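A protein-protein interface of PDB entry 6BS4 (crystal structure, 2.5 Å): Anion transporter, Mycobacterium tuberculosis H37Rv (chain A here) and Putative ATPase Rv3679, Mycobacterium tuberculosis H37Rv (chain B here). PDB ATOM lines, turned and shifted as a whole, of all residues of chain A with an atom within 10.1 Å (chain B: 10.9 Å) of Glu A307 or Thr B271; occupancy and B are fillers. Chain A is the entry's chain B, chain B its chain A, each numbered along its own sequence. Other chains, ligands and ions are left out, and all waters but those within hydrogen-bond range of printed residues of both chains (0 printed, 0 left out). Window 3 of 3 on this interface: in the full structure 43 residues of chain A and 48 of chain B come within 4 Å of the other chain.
Among the printed residues, pairs that only touch across the chains: Arg A296 with Gly B273 (3.7 Å), Arg A296 with Val B274 (3.8 Å), Ala A300 with Ala B272 (3.3 Å), Ala A300 with Val B274 (3.8 Å), Thr A303 with Ala B272 (3.7 Å), Leu A304 with Gly B268 (3.3 Å), Leu A304 with Thr B271 (3.9 Å), Leu A304 with Ala B272 (3.9 Å), Glu A307 with Thr B271 (3.7 Å), Ala A317 with Val B265 (3.96 Å), Ala A317 with Gly B268 (3.6 Å) and Leu A321 with Leu B269 (3.6 Å).
OG of Ser B264 sits at hydrogen-bond distance from OG1 of Thr A314 (3.3 Å).
Hydrophobic or aromatic side chains of chain A that line the printed part of chain B: Ala A300, Leu A304, Ala A317 and Leu A321. Among the printed residues, 13 pairs touch across the chains. Among the printed residues, no Asp or Glu carboxylate lies within 4 Å of a Lys or Arg side-chain nitrogen of the other chain.
OG1 of Thr B271 sits at hydrogen-bond distance from O of Ala B267 (3.3 Å). The backbone carbonyl oxygen of Leu B269 is in hydrogen-bond range of the backbone NH of Val B274 (2.8 Å). OG1 of Thr A303 lies within hydrogen-bond range of O of Ala A300 (3.2 Å).
Ala A301 touches none of the printed residues of chain B. Thr A303 touches just one residue of chain B: Ala B272. Leu A304 touches just these residues of chain B: Gly B268 (3.3 Å), Thr B271 (3.9 Å) and Ala B272 (3.9 Å). Of the printed residues of chain B, Glu A307 touches Thr B271. Printed residues of chain B within 4 Å of Thr A314: Ser B264 (3.3 Å). Printed residues of chain B within 4 Å of Leu A321: Leu B269. Asp B263 touches none of the printed residues of chain A. Printed residues of chain A within 4 Å of Ser B264: Thr A314 (3.3 Å). Printed residues of chain A within 4 Å of Val B265: Ala A317 (3.96 Å). Of chain A, only Leu A304 (3.3 Å) and Ala A317 (3.6 Å) come within 4 Å of Gly B268. Of the printed residues of chain A, Leu B269 touches Leu A321 (3.6 Å). Leu B270 touches none of the printed residues of chain A. Thr B271 touches two residues of chain A. The nearest residue of chain B that does not touch Glu A307 is Ala B272 (5.1 Å). The nearest residue of chain A that does not touch Thr B271 is Thr A303 (4.9 Å). The nearest printed residue of chain A that does not touch Gly B273 is Thr A303 (5.6 Å).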
ATOM      1  N   ARG A 296      25.987 -19.247   2.228  1.00  0.00           N
ATOM      2  CA  ARG A 296      26.479 -20.238   1.266  1.00  0.00           C
ATOM      3  C   ARG A 296      26.613 -19.629  -0.133  1.00  0.00           C
ATOM      4  O   ARG A 296      27.662 -19.782  -0.762  1.00  0.00           O
ATOM      5  CB  ARG A 296      25.529 -21.453   1.209  1.00  0.00           C
ATOM      6  CG  ARG A 296      25.814 -22.545   2.239  1.00  0.00           C
ATOM      7  CD  ARG A 296      26.602 -23.707   1.647  1.00  0.00           C
ATOM      8  NE  ARG A 296      25.780 -24.568   0.788  1.00  0.00           N
ATOM      9  CZ  ARG A 296      26.264 -25.493  -0.040  1.00  0.00           C
ATOM     10  NH1 ARG A 296      27.576 -25.684  -0.143  1.00  0.00           N
ATOM     11  NH2 ARG A 296      25.442 -26.227  -0.779  1.00  0.00           N
ATOM     12  N   ASP A 299      29.442 -16.930  -0.398  1.00  0.00           N
ATOM     13  CA  ASP A 299      30.730 -17.633  -0.446  1.00  0.00           C
ATOM     14  C   ASP A 299      30.955 -18.275  -1.811  1.00  0.00           C
ATOM     15  O   ASP A 299      32.030 -18.107  -2.380  1.00  0.00           O
ATOM     16  CB  ASP A 299      30.831 -18.703   0.665  1.00  0.00           C
ATOM     17  CG  ASP A 299      30.979 -18.172   2.080  1.00  0.00           C
ATOM     18  OD1 ASP A 299      31.624 -17.107   2.258  1.00  0.00           O
ATOM     19  OD2 ASP A 299      30.473 -18.831   3.014  1.00  0.00           O
ATOM     20  N   ALA A 300      29.932 -18.984  -2.346  1.00  0.00           N
ATOM     21  CA  ALA A 300      29.983 -19.653  -3.650  1.00  0.00           C
ATOM     22  C   ALA A 300      30.251 -18.659  -4.787  1.00  0.00           C
ATOM     23  O   ALA A 300      30.947 -19.000  -5.743  1.00  0.00           O
ATOM     24  CB  ALA A 300      28.696 -20.417  -3.902  1.00  0.00           C
ATOM     25  N   ALA A 301      29.737 -17.424  -4.660  1.00  0.00           N
ATOM     26  CA  ALA A 301      29.968 -16.353  -5.626  1.00  0.00           C
ATOM     27  C   ALA A 301      31.379 -15.781  -5.421  1.00  0.00           C
ATOM     28  O   ALA A 301      32.047 -15.460  -6.404  1.00  0.00           O
ATOM     29  CB  ALA A 301      28.923 -15.258  -5.452  1.00  0.00           C
ATOM     30  N   GLU A 302      31.831 -15.683  -4.146  1.00  0.00           N
ATOM     31  CA  GLU A 302      33.148 -15.164  -3.747  1.00  0.00           C
ATOM     32  C   GLU A 302      34.323 -16.017  -4.252  1.00  0.00           C
ATOM     33  O   GLU A 302      35.357 -15.457  -4.629  1.00  0.00           O
ATOM     34  CB  GLU A 302      33.232 -14.976  -2.221  1.00  0.00           C
ATOM     35  CG  GLU A 302      32.647 -13.663  -1.722  1.00  0.00           C
ATOM     36  CD  GLU A 302      32.682 -13.457  -0.217  1.00  0.00           C
ATOM     37  OE1 GLU A 302      32.153 -14.320   0.522  1.00  0.00           O
ATOM     38  OE2 GLU A 302      33.228 -12.420   0.221  1.00  0.00           O
ATOM     39  N   THR A 303      34.163 -17.363  -4.249  1.00  0.00           N
ATOM     40  CA  THR A 303      35.186 -18.307  -4.721  1.00  0.00           C
ATOM     41  C   THR A 303      35.338 -18.233  -6.243  1.00  0.00           C
ATOM     42  O   THR A 303      36.464 -18.274  -6.740  1.00  0.00           O
ATOM     43  CB  THR A 303      34.941 -19.754  -4.218  1.00  0.00           C
ATOM     44  OG1 THR A 303      33.740 -20.286  -4.776  1.00  0.00           O
ATOM     45  CG2 THR A 303      34.925 -19.868  -2.695  1.00  0.00           C
ATOM     46  N   LEU A 304      34.208 -18.098  -6.974  1.00  0.00           N
ATOM     47  CA  LEU A 304      34.160 -18.000  -8.438  1.00  0.00           C
ATOM     48  C   LEU A 304      34.860 -16.760  -8.999  1.00  0.00           C
ATOM     49  O   LEU A 304      35.378 -16.816 -10.117  1.00  0.00           O
ATOM     50  CB  LEU A 304      32.709 -18.073  -8.945  1.00  0.00           C
ATOM     51  CG  LEU A 304      32.071 -19.469  -8.997  1.00  0.00           C
ATOM     52  CD1 LEU A 304      30.558 -19.370  -9.113  1.00  0.00           C
ATOM     53  CD2 LEU A 304      32.638 -20.296 -10.151  1.00  0.00           C
ATOM     54  N   ASP A 305      34.876 -15.650  -8.226  1.00  0.00           N
ATOM     55  CA  ASP A 305      35.526 -14.385  -8.592  1.00  0.00           C
ATOM     56  C   ASP A 305      37.034 -14.567  -8.745  1.00  0.00           C
ATOM     57  O   ASP A 305      37.618 -14.031  -9.688  1.00  0.00           O
ATOM     58  CB  ASP A 305      35.243 -13.293  -7.540  1.00  0.00           C
ATOM     59  CG  ASP A 305      33.783 -12.915  -7.364  1.00  0.00           C
ATOM     60  OD1 ASP A 305      33.066 -12.814  -8.384  1.00  0.00           O
ATOM     61  OD2 ASP A 305      33.363 -12.698  -6.207  1.00  0.00           O
ATOM     62  N   ALA A 306      37.649 -15.339  -7.824  1.00  0.00           N
ATOM     63  CA  ALA A 306      39.085 -15.639  -7.791  1.00  0.00           C
ATOM     64  C   ALA A 306      39.464 -16.887  -8.626  1.00  0.00           C
ATOM     65  O   ALA A 306      40.621 -17.320  -8.602  1.00  0.00           O
ATOM     66  CB  ALA A 306      39.542 -15.800  -6.346  1.00  0.00           C
ATOM     67  N   GLU A 307      38.491 -17.448  -9.373  1.00  0.00           N
ATOM     68  CA  GLU A 307      38.663 -18.624 -10.231  1.00  0.00           C
ATOM     69  C   GLU A 307      38.059 -18.353 -11.611  1.00  0.00           C
ATOM     70  O   GLU A 307      38.180 -19.172 -12.521  1.00  0.00           O
ATOM     71  CB  GLU A 307      38.018 -19.868  -9.593  1.00  0.00           C
ATOM     72  CG  GLU A 307      38.752 -20.393  -8.369  1.00  0.00           C
ATOM     73  CD  GLU A 307      38.160 -21.638  -7.739  1.00  0.00           C
ATOM     74  OE1 GLU A 307      36.952 -21.627  -7.410  1.00  0.00           O
ATOM     75  OE2 GLU A 307      38.912 -22.623  -7.559  1.00  0.00           O
ATOM     76  N   THR A 314      33.893 -18.829 -17.442  1.00  0.00           N
ATOM     77  CA  THR A 314      32.552 -18.269 -17.230  1.00  0.00           C
ATOM     78  C   THR A 314      32.530 -17.323 -16.005  1.00  0.00           C
ATOM     79  O   THR A 314      33.518 -17.257 -15.266  1.00  0.00           O
ATOM     80  CB  THR A 314      31.487 -19.406 -17.190  1.00  0.00           C
ATOM     81  OG1 THR A 314      30.196 -18.873 -17.485  1.00  0.00           O
ATOM     82  CG2 THR A 314      31.458 -20.175 -15.864  1.00  0.00           C
ATOM     83  N   SER A 315      31.400 -16.590 -15.807  1.00  0.00           N
ATOM     84  CA  SER A 315      31.167 -15.634 -14.709  1.00  0.00           C
ATOM     85  C   SER A 315      29.664 -15.486 -14.385  1.00  0.00           C
ATOM     86  O   SER A 315      29.297 -14.818 -13.412  1.00  0.00           O
ATOM     87  CB  SER A 315      31.764 -14.272 -15.057  1.00  0.00           C
ATOM     88  OG  SER A 315      31.143 -13.707 -16.202  1.00  0.00           O
ATOM     89  N   ALA A 317      27.366 -17.861 -13.444  1.00  0.00           N
ATOM     90  CA  ALA A 317      26.990 -18.591 -12.230  1.00  0.00           C
ATOM     91  C   ALA A 317      27.149 -17.775 -10.936  1.00  0.00           C
ATOM     92  O   ALA A 317      26.344 -17.946 -10.019  1.00  0.00           O
ATOM     93  CB  ALA A 317      27.764 -19.893 -12.139  1.00  0.00           C
ATOM     94  N   ALA A 318      28.169 -16.888 -10.869  1.00  0.00           N
ATOM     95  CA  ALA A 318      28.396 -16.027  -9.706  1.00  0.00           C
ATOM     96  C   ALA A 318      27.317 -14.929  -9.633  1.00  0.00           C
ATOM     97  O   ALA A 318      26.785 -14.680  -8.551  1.00  0.00           O
ATOM     98  CB  ALA A 318      29.783 -15.412  -9.761  1.00  0.00           C
ATOM     99  N   LEU A 321      24.157 -16.403  -8.500  1.00  0.00           N
ATOM    100  CA  LEU A 321      24.276 -16.610  -7.062  1.00  0.00           C
ATOM    101  C   LEU A 321      24.104 -15.295  -6.312  1.00  0.00           C
ATOM    102  O   LEU A 321      23.561 -15.300  -5.205  1.00  0.00           O
ATOM    103  CB  LEU A 321      25.631 -17.277  -6.737  1.00  0.00           C
ATOM    104  CG  LEU A 321      25.894 -18.709  -7.257  1.00  0.00           C
ATOM    105  CD1 LEU A 321      27.321 -19.194  -6.991  1.00  0.00           C
ATOM    106  CD2 LEU A 321      24.899 -19.683  -6.670  1.00  0.00           C
ATOM    107  N   ASP B 263      23.289 -25.450 -18.281  1.00  0.00           N
ATOM    108  CA  ASP B 263      24.557 -26.175 -18.337  1.00  0.00           C
ATOM    109  C   ASP B 263      25.694 -25.313 -17.803  1.00  0.00           C
ATOM    110  O   ASP B 263      26.485 -25.748 -16.968  1.00  0.00           O
ATOM    111  CB  ASP B 263      24.858 -26.617 -19.770  1.00  0.00           C
ATOM    112  CG  ASP B 263      23.954 -27.741 -20.237  1.00  0.00           C
ATOM    113  OD1 ASP B 263      23.659 -28.644 -19.425  1.00  0.00           O
ATOM    114  OD2 ASP B 263      23.538 -27.721 -21.414  1.00  0.00           O
ATOM    115  N   SER B 264      25.760 -24.083 -18.299  1.00  0.00           N
ATOM    116  CA  SER B 264      26.779 -23.111 -17.870  1.00  0.00           C
ATOM    117  C   SER B 264      26.629 -22.731 -16.382  1.00  0.00           C
ATOM    118  O   SER B 264      27.642 -22.470 -15.722  1.00  0.00           O
ATOM    119  CB  SER B 264      26.737 -21.863 -18.748  1.00  0.00           C
ATOM    120  OG  SER B 264      27.745 -20.921 -18.410  1.00  0.00           O
ATOM    121  N   VAL B 265      25.368 -22.703 -15.865  1.00  0.00           N
ATOM    122  CA  VAL B 265      25.041 -22.401 -14.458  1.00  0.00           C
ATOM    123  C   VAL B 265      25.404 -23.612 -13.572  1.00  0.00           C
ATOM    124  O   VAL B 265      26.007 -23.426 -12.513  1.00  0.00           O
ATOM    125  CB  VAL B 265      23.572 -21.912 -14.261  1.00  0.00           C
ATOM    126  CG1 VAL B 265      23.215 -21.772 -12.783  1.00  0.00           C
ATOM    127  CG2 VAL B 265      23.332 -20.592 -14.980  1.00  0.00           C
ATOM    128  N   ARG B 266      25.068 -24.841 -14.029  1.00  0.00           N
ATOM    129  CA  ARG B 266      25.384 -26.108 -13.349  1.00  0.00           C
ATOM    130  C   ARG B 266      26.907 -26.285 -13.260  1.00  0.00           C
ATOM    131  O   ARG B 266      27.409 -26.729 -12.225  1.00  0.00           O
ATOM    132  CB  ARG B 266      24.751 -27.303 -14.087  1.00  0.00           C
ATOM    133  CG  ARG B 266      23.961 -28.243 -13.176  1.00  0.00           C
ATOM    134  CD  ARG B 266      23.468 -29.500 -13.888  1.00  0.00           C
ATOM    135  NE  ARG B 266      22.482 -29.222 -14.941  1.00  0.00           N
ATOM    136  CZ  ARG B 266      21.170 -29.108 -14.744  1.00  0.00           C
ATOM    137  NH1 ARG B 266      20.659 -29.234 -13.523  1.00  0.00           N
ATOM    138  NH2 ARG B 266      20.359 -28.853 -15.763  1.00  0.00           N
ATOM    139  N   ALA B 267      27.633 -25.893 -14.340  1.00  0.00           N
ATOM    140  CA  ALA B 267      29.092 -25.952 -14.456  1.00  0.00           C
ATOM    141  C   ALA B 267      29.777 -25.024 -13.454  1.00  0.00           C
ATOM    142  O   ALA B 267      30.678 -25.463 -12.738  1.00  0.00           O
ATOM    143  CB  ALA B 267      29.524 -25.604 -15.875  1.00  0.00           C
ATOM    144  N   GLY B 268      29.334 -23.768 -13.404  1.00  0.00           N
ATOM    145  CA  GLY B 268      29.864 -22.763 -12.491  1.00  0.00           C
ATOM    146  C   GLY B 268      29.564 -23.059 -11.034  1.00  0.00           C
ATOM    147  O   GLY B 268      30.286 -22.596 -10.150  1.00  0.00           O
ATOM    148  N   LEU B 269      28.498 -23.841 -10.769  1.00  0.00           N
ATOM    149  CA  LEU B 269      28.126 -24.235  -9.413  1.00  0.00           C
ATOM    150  C   LEU B 269      29.030 -25.361  -8.904  1.00  0.00           C
ATOM    151  O   LEU B 269      29.294 -25.422  -7.701  1.00  0.00           O
ATOM    152  CB  LEU B 269      26.638 -24.608  -9.316  1.00  0.00           C
ATOM    153  CG  LEU B 269      25.666 -23.433  -9.118  1.00  0.00           C
ATOM    154  CD1 LEU B 269      24.290 -23.763  -9.651  1.00  0.00           C
ATOM    155  CD2 LEU B 269      25.560 -23.039  -7.659  1.00  0.00           C
ATOM    156  N   LEU B 270      29.533 -26.221  -9.821  1.00  0.00           N
ATOM    157  CA  LEU B 270      30.457 -27.322  -9.510  1.00  0.00           C
ATOM    158  C   LEU B 270      31.804 -26.765  -9.027  1.00  0.00           C
ATOM    159  O   LEU B 270      32.339 -27.242  -8.025  1.00  0.00           O
ATOM    160  CB  LEU B 270      30.665 -28.233 -10.737  1.00  0.00           C
ATOM    161  CG  LEU B 270      29.540 -29.214 -11.082  1.00  0.00           C
ATOM    162  CD1 LEU B 270      29.558 -29.555 -12.557  1.00  0.00           C
ATOM    163  CD2 LEU B 270      29.642 -30.490 -10.256  1.00  0.00           C
ATOM    164  N   THR B 271      32.321 -25.730  -9.727  1.00  0.00           N
ATOM    165  CA  THR B 271      33.565 -25.003  -9.439  1.00  0.00           C
ATOM    166  C   THR B 271      33.509 -24.357  -8.036  1.00  0.00           C
ATOM    167  O   THR B 271      34.513 -24.349  -7.326  1.00  0.00           O
ATOM    168  CB  THR B 271      33.815 -23.959 -10.552  1.00  0.00           C
ATOM    169  OG1 THR B 271      33.742 -24.604 -11.825  1.00  0.00           O
ATOM    170  CG2 THR B 271      35.157 -23.232 -10.415  1.00  0.00           C
ATOM    171  N   ALA B 272      32.324 -23.842  -7.643  1.00  0.00           N
ATOM    172  CA  ALA B 272      32.061 -23.191  -6.352  1.00  0.00           C
ATOM    173  C   ALA B 272      31.787 -24.188  -5.201  1.00  0.00           C
ATOM    174  O   ALA B 272      31.620 -23.767  -4.051  1.00  0.00           O
ATOM    175  CB  ALA B 272      30.896 -22.224  -6.496  1.00  0.00           C
ATOM    176  N   GLY B 273      31.761 -25.484  -5.527  1.00  0.00           N
ATOM    177  CA  GLY B 273      31.501 -26.563  -4.580  1.00  0.00           C
ATOM    178  C   GLY B 273      30.060 -26.581  -4.112  1.00  0.00           C
ATOM    179  O   GLY B 273      29.800 -26.642  -2.905  1.00  0.00           O
ATOM    180  N   VAL B 274      29.111 -26.472  -5.074  1.00  0.00           N
ATOM    181  CA  VAL B 274      27.662 -26.456  -4.828  1.00  0.00           C
ATOM    182  C   VAL B 274      26.935 -27.352  -5.856  1.00  0.00           C
ATOM    183  O   VAL B 274      27.057 -27.147  -7.067  1.00  0.00           O
ATOM    184  CB  VAL B 274      27.054 -25.013  -4.787  1.00  0.00           C
ATOM    185  CG1 VAL B 274      25.572 -25.042  -4.417  1.00  0.00           C
ATOM    186  CG2 VAL B 274      27.818 -24.089  -3.837  1.00  0.00           C
ATOM    187  N   LYS B 275      26.184 -28.344  -5.353  1.00  0.00           N
ATOM    188  CA  LYS B 275      25.366 -29.260  -6.149  1.00  0.00           C
ATOM    189  C   LYS B 275      23.936 -29.036  -5.681  1.00  0.00           C
ATOM    190  O   LYS B 275      23.659 -29.094  -4.478  1.00  0.00           O
ATOM    191  CB  LYS B 275      25.802 -30.723  -5.948  1.00  0.00           C
ATOM    192  CG  LYS B 275      25.307 -31.669  -7.041  1.00  0.00           C
ATOM    193  CD  LYS B 275      25.824 -33.085  -6.838  1.00  0.00           C
ATOM    194  CE  LYS B 275      25.446 -34.000  -7.979  1.00  0.00           C
ATOM    195  NZ  LYS B 275      25.996 -35.371  -7.798  1.00  0.00           N
ATOM    196  N   LEU B 276      23.040 -28.721  -6.619  1.00  0.00           N
ATOM    197  CA  LEU B 276      21.658 -28.389  -6.292  1.00  0.00           C
ATOM    198  C   LEU B 276      20.628 -29.394  -6.819  1.00  0.00           C
ATOM    199  O   LEU B 276      20.738 -29.811  -7.978  1.00  0.00           O
ATOM    200  CB  LEU B 276      21.352 -26.986  -6.850  1.00  0.00           C
ATOM    201  CG  LEU B 276      20.790 -25.935  -5.900  1.00  0.00           C
ATOM    202  CD1 LEU B 276      21.827 -25.487  -4.874  1.00  0.00           C
ATOM    203  CD2 LEU B 276      20.346 -24.727  -6.675  1.00  0.00           C
ATOM    204  N   PHE B 281      17.258 -26.019  -8.361  1.00  0.00           N
ATOM    205  CA  PHE B 281      18.013 -25.523  -9.513  1.00  0.00           C
ATOM    206  C   PHE B 281      17.079 -24.754 -10.437  1.00  0.00           C
ATOM    207  O   PHE B 281      17.449 -23.678 -10.906  1.00  0.00           O
ATOM    208  CB  PHE B 281      18.738 -26.668 -10.264  1.00  0.00           C
ATOM    209  CG  PHE B 281      19.685 -26.161 -11.328  1.00  0.00           C
ATOM    210  CD1 PHE B 281      20.927 -25.632 -10.986  1.00  0.00           C
ATOM    211  CD2 PHE B 281      19.319 -26.169 -12.669  1.00  0.00           C
ATOM    212  CE1 PHE B 281      21.788 -25.130 -11.968  1.00  0.00           C
ATOM    213  CE2 PHE B 281      20.184 -25.670 -13.649  1.00  0.00           C
ATOM    214  CZ  PHE B 281      21.408 -25.149 -13.291  1.00  0.00           C
